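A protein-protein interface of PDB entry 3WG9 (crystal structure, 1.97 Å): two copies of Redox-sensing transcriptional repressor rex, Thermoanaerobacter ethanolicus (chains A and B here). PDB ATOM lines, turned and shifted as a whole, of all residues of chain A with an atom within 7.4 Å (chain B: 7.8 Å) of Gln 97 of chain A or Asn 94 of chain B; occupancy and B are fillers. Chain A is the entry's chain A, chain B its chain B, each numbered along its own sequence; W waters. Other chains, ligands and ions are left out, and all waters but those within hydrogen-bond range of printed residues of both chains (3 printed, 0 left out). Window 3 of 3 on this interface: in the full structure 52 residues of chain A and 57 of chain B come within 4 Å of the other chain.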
ATOM      1  N   ILE A  89      21.686  10.613  -1.635  1.00  0.00           N
ATOM      2  CA  ILE A  89      21.163   9.394  -1.033  1.00  0.00           C
ATOM      3  C   ILE A  89      21.800   9.166   0.301  1.00  0.00           C
ATOM      4  O   ILE A  89      23.053   9.256   0.430  1.00  0.00           O
ATOM      5  CB  ILE A  89      21.443   8.215  -1.947  1.00  0.00           C
ATOM      6  CG1 ILE A  89      20.567   8.345  -3.205  1.00  0.00           C
ATOM      7  CG2 ILE A  89      21.204   6.835  -1.251  1.00  0.00           C
ATOM      8  CD1 ILE A  89      21.040   7.327  -4.364  1.00  0.00           C
ATOM      9  N   GLY A  91      22.390   6.356   3.073  1.00  0.00           N
ATOM     10  CA  GLY A  91      22.401   4.877   3.166  1.00  0.00           C
ATOM     11  C   GLY A  91      23.044   4.254   1.931  1.00  0.00           C
ATOM     12  O   GLY A  91      22.485   4.324   0.812  1.00  0.00           O
ATOM     13  N   ALA A  92      24.196   3.608   2.105  1.00  0.00           N
ATOM     14  CA  ALA A  92      24.876   2.986   0.967  1.00  0.00           C
ATOM     15  C   ALA A  92      24.741   1.459   0.964  1.00  0.00           C
ATOM     16  O   ALA A  92      25.606   0.745   0.440  1.00  0.00           O
ATOM     17  CB  ALA A  92      26.352   3.421   0.917  1.00  0.00           C
ATOM     18  N   GLY A  93      23.691   0.943   1.598  1.00  0.00           N
ATOM     19  CA  GLY A  93      23.400  -0.486   1.569  1.00  0.00           C
ATOM     20  C   GLY A  93      22.837  -0.934   0.242  1.00  0.00           C
ATOM     21  O   GLY A  93      22.920  -0.189  -0.753  1.00  0.00           O
ATOM     22  N   ASN A  94      22.278  -2.171   0.157  1.00  0.00           N
ATOM     23  CA  ASN A  94      21.819  -2.598  -1.193  1.00  0.00           C
ATOM     24  C   ASN A  94      20.760  -1.650  -1.828  1.00  0.00           C
ATOM     25  O   ASN A  94      20.831  -1.282  -2.981  1.00  0.00           O
ATOM     26  CB  ASN A  94      21.292  -4.023  -1.151  1.00  0.00           C
ATOM     27  CG  ASN A  94      22.423  -5.023  -0.987  1.00  0.00           C
ATOM     28  OD1 ASN A  94      23.300  -5.136  -1.830  1.00  0.00           O
ATOM     29  ND2 ASN A  94      22.397  -5.728   0.082  1.00  0.00           N
ATOM     30  N   LEU A  95      19.796  -1.246  -1.027  1.00  0.00           N
ATOM     31  CA  LEU A  95      18.716  -0.365  -1.547  1.00  0.00           C
ATOM     32  C   LEU A  95      19.282   0.986  -2.008  1.00  0.00           C
ATOM     33  O   LEU A  95      19.075   1.445  -3.143  1.00  0.00           O
ATOM     34  CB  LEU A  95      17.666  -0.190  -0.439  1.00  0.00           C
ATOM     35  CG  LEU A  95      16.566   0.832  -0.756  1.00  0.00           C
ATOM     36  CD1 LEU A  95      15.805   0.419  -2.031  1.00  0.00           C
ATOM     37  CD2 LEU A  95      15.754   1.084   0.504  1.00  0.00           C
ATOM     38  N   GLY A  96      20.092   1.616  -1.140  1.00  0.00           N
ATOM     39  CA  GLY A  96      20.793   2.828  -1.589  1.00  0.00           C
ATOM     40  C   GLY A  96      21.558   2.705  -2.872  1.00  0.00           C
ATOM     41  O   GLY A  96      21.529   3.598  -3.732  1.00  0.00           O
ATOM     42  N   GLN A  97      22.308   1.614  -3.023  1.00  0.00           N
ATOM     43  CA  GLN A  97      23.107   1.470  -4.239  1.00  0.00           C
ATOM     44  C   GLN A  97      22.210   1.176  -5.425  1.00  0.00           C
ATOM     45  O   GLN A  97      22.424   1.682  -6.534  1.00  0.00           O
ATOM     46  CB  GLN A  97      24.087   0.286  -4.065  1.00  0.00           C
ATOM     47  CG  GLN A  97      25.211   0.584  -3.072  1.00  0.00           C
ATOM     48  CD  GLN A  97      26.210  -0.573  -2.969  1.00  0.00           C
ATOM     49  OE1 GLN A  97      26.674  -1.092  -3.968  1.00  0.00           O
ATOM     50  NE2 GLN A  97      26.454  -1.018  -1.763  1.00  0.00           N
ATOM     51  N   ALA A  98      21.156   0.397  -5.158  1.00  0.00           N
ATOM     52  CA  ALA A  98      20.131   0.135  -6.201  1.00  0.00           C
ATOM     53  C   ALA A  98      19.564   1.463  -6.709  1.00  0.00           C
ATOM     54  O   ALA A  98      19.432   1.708  -7.906  1.00  0.00           O
ATOM     55  CB  ALA A  98      18.995  -0.769  -5.571  1.00  0.00           C
ATOM     56  N   ILE A  99      19.260   2.374  -5.781  1.00  0.00           N
ATOM     57  CA  ILE A  99      18.659   3.613  -6.208  1.00  0.00           C
ATOM     58  C   ILE A  99      19.698   4.509  -6.935  1.00  0.00           C
ATOM     59  O   ILE A  99      19.383   5.202  -7.915  1.00  0.00           O
ATOM     60  CB  ILE A  99      18.033   4.388  -4.999  1.00  0.00           C
ATOM     61  CG1 ILE A  99      16.921   3.580  -4.306  1.00  0.00           C
ATOM     62  CG2 ILE A  99      17.483   5.740  -5.473  1.00  0.00           C
ATOM     63  CD1 ILE A  99      15.858   3.003  -5.302  1.00  0.00           C
ATOM     64  N   ALA A 100      20.936   4.518  -6.456  1.00  0.00           N
ATOM     65  CA  ALA A 100      21.991   5.281  -7.154  1.00  0.00           C
ATOM     66  C   ALA A 100      22.151   4.781  -8.601  1.00  0.00           C
ATOM     67  O   ALA A 100      22.323   5.580  -9.531  1.00  0.00           O
ATOM     68  CB  ALA A 100      23.345   5.163  -6.390  1.00  0.00           C
ATOM     69  N   ASN A 101      22.053   3.462  -8.781  1.00  0.00           N
ATOM     70  CA  ASN A 101      22.244   2.853 -10.098  1.00  0.00           C
ATOM     71  C   ASN A 101      20.961   2.782 -10.907  1.00  0.00           C
ATOM     72  O   ASN A 101      20.974   2.184 -11.994  1.00  0.00           O
ATOM     73  CB  ASN A 101      22.871   1.434  -9.970  1.00  0.00           C
ATOM     74  CG  ASN A 101      24.375   1.485  -9.627  1.00  0.00           C
ATOM     75  OD1 ASN A 101      25.179   1.961 -10.426  1.00  0.00           O
ATOM     76  ND2 ASN A 101      24.735   1.073  -8.410  1.00  0.00           N
ATOM     77  N   TYR A 102      19.874   3.369 -10.394  1.00  0.00           N
ATOM     78  CA  TYR A 102      18.603   3.451 -11.145  1.00  0.00           C
ATOM     79  C   TYR A 102      18.652   4.630 -12.107  1.00  0.00           C
ATOM     80  O   TYR A 102      17.978   5.641 -11.901  1.00  0.00           O
ATOM     81  CB  TYR A 102      17.356   3.548 -10.224  1.00  0.00           C
ATOM     82  CG  TYR A 102      16.112   2.800 -10.721  1.00  0.00           C
ATOM     83  CD1 TYR A 102      15.950   1.421 -10.503  1.00  0.00           C
ATOM     84  CD2 TYR A 102      15.114   3.470 -11.424  1.00  0.00           C
ATOM     85  CE1 TYR A 102      14.799   0.729 -10.973  1.00  0.00           C
ATOM     86  CE2 TYR A 102      13.958   2.809 -11.897  1.00  0.00           C
ATOM     87  CZ  TYR A 102      13.804   1.439 -11.646  1.00  0.00           C
ATOM     88  OH  TYR A 102      12.701   0.786 -12.155  1.00  0.00           O
ATOM     89  N   ILE A 115      26.521  10.425  -1.923  1.00  0.00           N
ATOM     90  CA  ILE A 115      25.910   9.309  -1.188  1.00  0.00           C
ATOM     91  C   ILE A 115      26.511   9.351   0.211  1.00  0.00           C
ATOM     92  O   ILE A 115      27.701   9.690   0.316  1.00  0.00           O
ATOM     93  CB  ILE A 115      26.256   7.976  -1.903  1.00  0.00           C
ATOM     94  CG1 ILE A 115      25.602   7.931  -3.291  1.00  0.00           C
ATOM     95  CG2 ILE A 115      25.758   6.799  -1.096  1.00  0.00           C
ATOM     96  CD1 ILE A 115      26.222   6.817  -4.212  1.00  0.00           C
ATOM     97  N   LEU A 122      33.377   2.352   4.074  1.00  0.00           N
ATOM     98  CA  LEU A 122      32.907   2.735   2.735  1.00  0.00           C
ATOM     99  C   LEU A 122      33.382   4.115   2.260  1.00  0.00           C
ATOM    100  O   LEU A 122      33.192   4.464   1.072  1.00  0.00           O
ATOM    101  CB  LEU A 122      31.347   2.751   2.694  1.00  0.00           C
ATOM    102  CG  LEU A 122      30.633   1.460   3.100  1.00  0.00           C
ATOM    103  CD1 LEU A 122      29.137   1.700   2.977  1.00  0.00           C
ATOM    104  CD2 LEU A 122      31.046   0.365   2.161  1.00  0.00           C
ATOM    105  N   LYS A 126      33.386   4.906  -4.642  1.00  0.00           N
ATOM    106  CA  LYS A 126      32.566   5.643  -5.598  1.00  0.00           C
ATOM    107  C   LYS A 126      31.515   4.682  -6.170  1.00  0.00           C
ATOM    108  O   LYS A 126      31.750   3.488  -6.257  1.00  0.00           O
ATOM    109  CB  LYS A 126      33.420   6.240  -6.725  1.00  0.00           C
ATOM    110  CG  LYS A 126      34.556   7.120  -6.255  1.00  0.00           C
ATOM    111  CD  LYS A 126      34.821   8.314  -7.189  1.00  0.00           C
ATOM    112  CE  LYS A 126      35.643   7.952  -8.428  1.00  0.00           C
ATOM    113  NZ  LYS A 126      37.113   8.258  -8.282  1.00  0.00           N
ATOM    114  N   ILE A 127      30.325   5.197  -6.460  1.00  0.00           N
ATOM    115  CA  ILE A 127      29.289   4.435  -7.170  1.00  0.00           C
ATOM    116  C   ILE A 127      28.879   5.362  -8.281  1.00  0.00           C
ATOM    117  O   ILE A 127      28.428   6.481  -8.022  1.00  0.00           O
ATOM    118  CB  ILE A 127      28.069   4.150  -6.269  1.00  0.00           C
ATOM    119  CG1 ILE A 127      28.437   3.151  -5.189  1.00  0.00           C
ATOM    120  CG2 ILE A 127      26.879   3.645  -7.092  1.00  0.00           C
ATOM    121  CD1 ILE A 127      27.651   3.328  -3.922  1.00  0.00           C
ATOM    122  N   ARG A 128      29.136   4.933  -9.510  1.00  0.00           N
ATOM    123  CA  ARG A 128      28.918   5.774 -10.683  1.00  0.00           C
ATOM    124  C   ARG A 128      29.609   7.132 -10.584  1.00  0.00           C
ATOM    125  O   ARG A 128      29.000   8.169 -10.866  1.00  0.00           O
ATOM    126  CB  ARG A 128      27.413   5.988 -10.885  1.00  0.00           C
ATOM    127  CG  ARG A 128      26.641   4.843 -11.546  1.00  0.00           C
ATOM    128  CD  ARG A 128      25.300   5.357 -12.095  1.00  0.00           C
ATOM    129  NE  ARG A 128      24.915   6.598 -11.419  1.00  0.00           N
ATOM    130  CZ  ARG A 128      24.997   7.813 -11.956  1.00  0.00           C
ATOM    131  NH1 ARG A 128      24.684   8.876 -11.224  1.00  0.00           N
ATOM    132  NH2 ARG A 128      25.380   7.972 -13.219  1.00  0.00           N
ATOM    133  N   VAL A 132      31.012   8.070  -1.814  1.00  0.00           N
ATOM    134  CA  VAL A 132      30.359   7.727  -0.564  1.00  0.00           C
ATOM    135  C   VAL A 132      31.085   8.542   0.526  1.00  0.00           C
ATOM    136  O   VAL A 132      32.322   8.453   0.638  1.00  0.00           O
ATOM    137  CB  VAL A 132      30.432   6.201  -0.271  1.00  0.00           C
ATOM    138  CG1 VAL A 132      29.813   5.875   1.109  1.00  0.00           C
ATOM    139  CG2 VAL A 132      29.750   5.391  -1.401  1.00  0.00           C
ATOM    140  N   CYS A 153      17.504   5.831   2.437  1.00  0.00           N
ATOM    141  CA  CYS A 153      17.650   4.365   2.265  1.00  0.00           C
ATOM    142  C   CYS A 153      18.418   3.803   3.461  1.00  0.00           C
ATOM    143  O   CYS A 153      19.320   2.973   3.336  1.00  0.00           O
ATOM    144  CB  CYS A 153      18.413   4.025   0.976  1.00  0.00           C
ATOM    145  SG  CYS A 153      17.623   4.745  -0.527  1.00  0.00           S
ATOM    146  N   GLY B  91      17.922 -11.723 -10.754  1.00  0.00           N
ATOM    147  CA  GLY B  91      18.884 -10.581 -10.579  1.00  0.00           C
ATOM    148  C   GLY B  91      19.428 -10.607  -9.155  1.00  0.00           C
ATOM    149  O   GLY B  91      18.656 -10.461  -8.201  1.00  0.00           O
ATOM    150  N   ALA B  92      20.722 -10.876  -8.987  1.00  0.00           N
ATOM    151  CA  ALA B  92      21.311 -10.915  -7.658  1.00  0.00           C
ATOM    152  C   ALA B  92      22.195  -9.707  -7.348  1.00  0.00           C
ATOM    153  O   ALA B  92      22.891  -9.753  -6.365  1.00  0.00           O
ATOM    154  CB  ALA B  92      22.132 -12.203  -7.418  1.00  0.00           C
ATOM    155  N   GLY B  93      22.080  -8.632  -8.123  1.00  0.00           N
ATOM    156  CA  GLY B  93      22.649  -7.305  -7.766  1.00  0.00           C
ATOM    157  C   GLY B  93      21.970  -6.616  -6.602  1.00  0.00           C
ATOM    158  O   GLY B  93      21.134  -7.201  -5.898  1.00  0.00           O
ATOM    159  N   ASN B  94      22.334  -5.348  -6.385  1.00  0.00           N
ATOM    160  CA  ASN B  94      21.822  -4.604  -5.236  1.00  0.00           C
ATOM    161  C   ASN B  94      20.287  -4.597  -5.156  1.00  0.00           C
ATOM    162  O   ASN B  94      19.731  -4.849  -4.103  1.00  0.00           O
ATOM    163  CB  ASN B  94      22.347  -3.156  -5.319  1.00  0.00           C
ATOM    164  CG  ASN B  94      23.879  -3.119  -5.264  1.00  0.00           C
ATOM    165  OD1 ASN B  94      24.514  -2.600  -6.161  1.00  0.00           O
ATOM    166  ND2 ASN B  94      24.456  -3.698  -4.213  1.00  0.00           N
ATOM    167  N   LEU B  95      19.632  -4.299  -6.269  1.00  0.00           N
ATOM    168  CA  LEU B  95      18.160  -4.266  -6.315  1.00  0.00           C
ATOM    169  C   LEU B  95      17.586  -5.615  -5.854  1.00  0.00           C
ATOM    170  O   LEU B  95      16.788  -5.648  -4.916  1.00  0.00           O
ATOM    171  CB  LEU B  95      17.688  -3.883  -7.723  1.00  0.00           C
ATOM    172  CG  LEU B  95      16.134  -3.793  -7.833  1.00  0.00           C
ATOM    173  CD1 LEU B  95      15.564  -2.809  -6.810  1.00  0.00           C
ATOM    174  CD2 LEU B  95      15.732  -3.397  -9.281  1.00  0.00           C
ATOM    175  N   GLY B  96      18.034  -6.735  -6.454  1.00  0.00           N
ATOM    176  CA  GLY B  96      17.501  -8.056  -6.079  1.00  0.00           C
ATOM    177  C   GLY B  96      17.726  -8.377  -4.610  1.00  0.00           C
ATOM    178  O   GLY B  96      16.836  -8.899  -3.932  1.00  0.00           O
ATOM    179  N   GLN B  97      18.920  -8.068  -4.085  1.00  0.00           N
ATOM    180  CA  GLN B  97      19.158  -8.276  -2.652  1.00  0.00           C
ATOM    181  C   GLN B  97      18.247  -7.400  -1.804  1.00  0.00           C
ATOM    182  O   GLN B  97      17.764  -7.835  -0.742  1.00  0.00           O
ATOM    183  CB  GLN B  97      20.649  -8.007  -2.322  1.00  0.00           C
ATOM    184  CG  GLN B  97      21.570  -8.959  -3.145  1.00  0.00           C
ATOM    185  CD  GLN B  97      23.048  -8.762  -2.824  1.00  0.00           C
ATOM    186  OE1 GLN B  97      23.395  -8.725  -1.654  1.00  0.00           O
ATOM    187  NE2 GLN B  97      23.883  -8.513  -3.838  1.00  0.00           N
ATOM    188  N   ALA B  98      17.988  -6.173  -2.250  1.00  0.00           N
ATOM    189  CA  ALA B  98      17.141  -5.275  -1.406  1.00  0.00           C
ATOM    190  C   ALA B  98      15.719  -5.805  -1.400  1.00  0.00           C
ATOM    191  O   ALA B  98      14.978  -5.699  -0.396  1.00  0.00           O
ATOM    192  CB  ALA B  98      17.134  -3.848  -1.970  1.00  0.00           C
ATOM    193  N   ILE B  99      15.284  -6.275  -2.578  1.00  0.00           N
ATOM    194  CA  ILE B  99      13.927  -6.832  -2.641  1.00  0.00           C
ATOM    195  C   ILE B  99      13.859  -8.145  -1.874  1.00  0.00           C
ATOM    196  O   ILE B  99      12.876  -8.416  -1.166  1.00  0.00           O
ATOM    197  CB  ILE B  99      13.413  -6.967  -4.079  1.00  0.00           C
ATOM    198  CG1 ILE B  99      13.376  -5.591  -4.729  1.00  0.00           C
ATOM    199  CG2 ILE B  99      11.962  -7.623  -4.090  1.00  0.00           C
ATOM    200  CD1 ILE B  99      12.688  -4.483  -3.874  1.00  0.00           C
ATOM    201  N   ALA B 100      14.920  -8.952  -1.944  1.00  0.00           N
ATOM    202  CA  ALA B 100      14.983 -10.139  -1.128  1.00  0.00           C
ATOM    203  C   ALA B 100      14.845  -9.769   0.359  1.00  0.00           C
ATOM    204  O   ALA B 100      14.048 -10.383   1.077  1.00  0.00           O
ATOM    205  CB  ALA B 100      16.279 -10.921  -1.401  1.00  0.00           C
ATOM    206  N   ASN B 101      15.564  -8.740   0.812  1.00  0.00           N
ATOM    207  CA  ASN B 101      15.435  -8.225   2.198  1.00  0.00           C
ATOM    208  C   ASN B 101      14.006  -7.710   2.491  1.00  0.00           C
ATOM    209  O   ASN B 101      13.436  -7.998   3.536  1.00  0.00           O
ATOM    210  CB  ASN B 101      16.475  -7.104   2.505  1.00  0.00           C
ATOM    211  CG  ASN B 101      17.957  -7.536   2.307  1.00  0.00           C
ATOM    212  OD1 ASN B 101      18.870  -6.670   2.133  1.00  0.00           O
ATOM    213  ND2 ASN B 101      18.215  -8.847   2.376  1.00  0.00           N
ATOM    214  N   CYS B 153      14.511  -8.177 -11.337  1.00  0.00           N
ATOM    215  CA  CYS B 153      15.430  -7.130 -10.814  1.00  0.00           C
ATOM    216  C   CYS B 153      16.711  -7.132 -11.663  1.00  0.00           C
ATOM    217  O   CYS B 153      17.835  -7.075 -11.160  1.00  0.00           O
ATOM    218  CB  CYS B 153      15.779  -7.524  -9.380  1.00  0.00           C
ATOM    219  SG  CYS B 153      14.349  -7.418  -8.256  1.00  0.00           S
HETATM  220  O   HOH W   1      23.492  -1.450  -8.320  1.00  0.00           O
HETATM  221  O   HOH W   2      27.480  -3.474  -4.557  1.00  0.00           O
HETATM  222  O   HOH W   3      26.903  -0.518  -6.699  1.00  0.00           O
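The side-chain amide nitrogen of Asn 94 of chain B lies within hydrogen-bond range of the side-chain amide oxygen of Asn 94 of chain A, at 3.0 Å.
OD1 of Asn 94 of chain B sits close to OE1 of Gln 97 of chain A.
The side-chain amide nitrogen of Gln 97 of chain A lies within hydrogen-bond range of the backbone carbonyl oxygen of Ala 92 of chain A.
O of Gln 97 of chain A lies within hydrogen-bond range of ND2 of Asn 101 of chain A, 3.0 Å away.
The backbone carbonyl oxygen of Ala 92 of chain B lies within hydrogen-bond range of the side-chain amide nitrogen of Gln 97 of chain B (3.0 Å).
O of Gln 97 of chain B sits close to OD1 of Asn 101 of chain B.
Asn 94 of chain A touches Gln 97 of chain B.
Ala 98 of chain B touches Leu 95 of chain A (CB to N, 3.8 Å).
Ala 98 of chain A touches Asn 94 of chain B.
N of Leu 95 of chain B touches CB of Ala 98 of chain A, at 3.7 Å.
Of chain B, only Asn 94 (3.4 Å) comes within 4 Å of Gln 97 of chain A.
Of chain A, only Asn 94 (3.0 Å), Gln 97 (3.4 Å) and Ala 98 (3.8 Å) come within 4 Å of Asn 94 of chain B.
Gly 96 of chain A touches none of the printed residues of chain B.
Of the printed residues of chain B, Asn 94 of chain A touches Asn 94 (3.0 Å) and Gln 97 (3.6 Å).
Of the printed residues of chain A, Ala 98 of chain B touches Leu 95.
Printed residues of chain A within 4 Å of Gln 97 of chain B: Asn 94 (3.6 Å).
Of the printed residues of chain B, Leu 95 of chain A touches Ala 98 (3.8 Å).
Cys 153 of chain B touches none of the printed residues of chain A.
The nearest residue of chain B that does not touch Gln 97 of chain A is Leu 95 of chain B (6.1 Å).
The nearest residue of chain A that does not touch Asn 94 of chain B is Asn 101 of chain A (4.3 Å).
The nearest printed residue of chain B that does not touch Leu 95 of chain A is Asn 94 of chain B (4.7 Å).
Hydrophobic or aromatic side chains of chain B that line the printed part of chain A: Ala 98.
Among the printed residues, 6 pairs touch across the chains.
Among the printed residues, no Asp or Glu carboxylate lies within 4 Å of a Lys or Arg side-chain nitrogen of the other chain.
Asn 94 of chain B touches its own counterpart, Asn 94 of chain A.
Asn 94 of chain A touches Gln 97 of chain B, and with the chains exchanged Gln 97 of chain A touches Asn 94 of chain B.
Leu 95 of chain A touches Ala 98 of chain B, and with the chains exchanged Ala 98 of chain A touches Leu 95 of chain B.
Ala 98 of chain A touches Asn 94 of chain B, but with the chains exchanged Asn 94 of chain A does not touch Ala 98 of chain B (4.1 Å).
Water W2 lies within hydrogen-bond range of OE1 of Gln 97 of chain A (2.6 Å) and ND2 of Asn 94 of chain B (3.1 Å).
Water W1 lies within hydrogen-bond range of OD1 of Asn 94 of chain B and ND2 of Asn 101 of chain A.
Water W3 lies within hydrogen-bond range of OE1 of Gln 97 of chain A (2.8 Å), ND2 of Asn 101 of chain A (3.2 Å) and OD1 of Asn 94 of chain B (3.2 Å).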
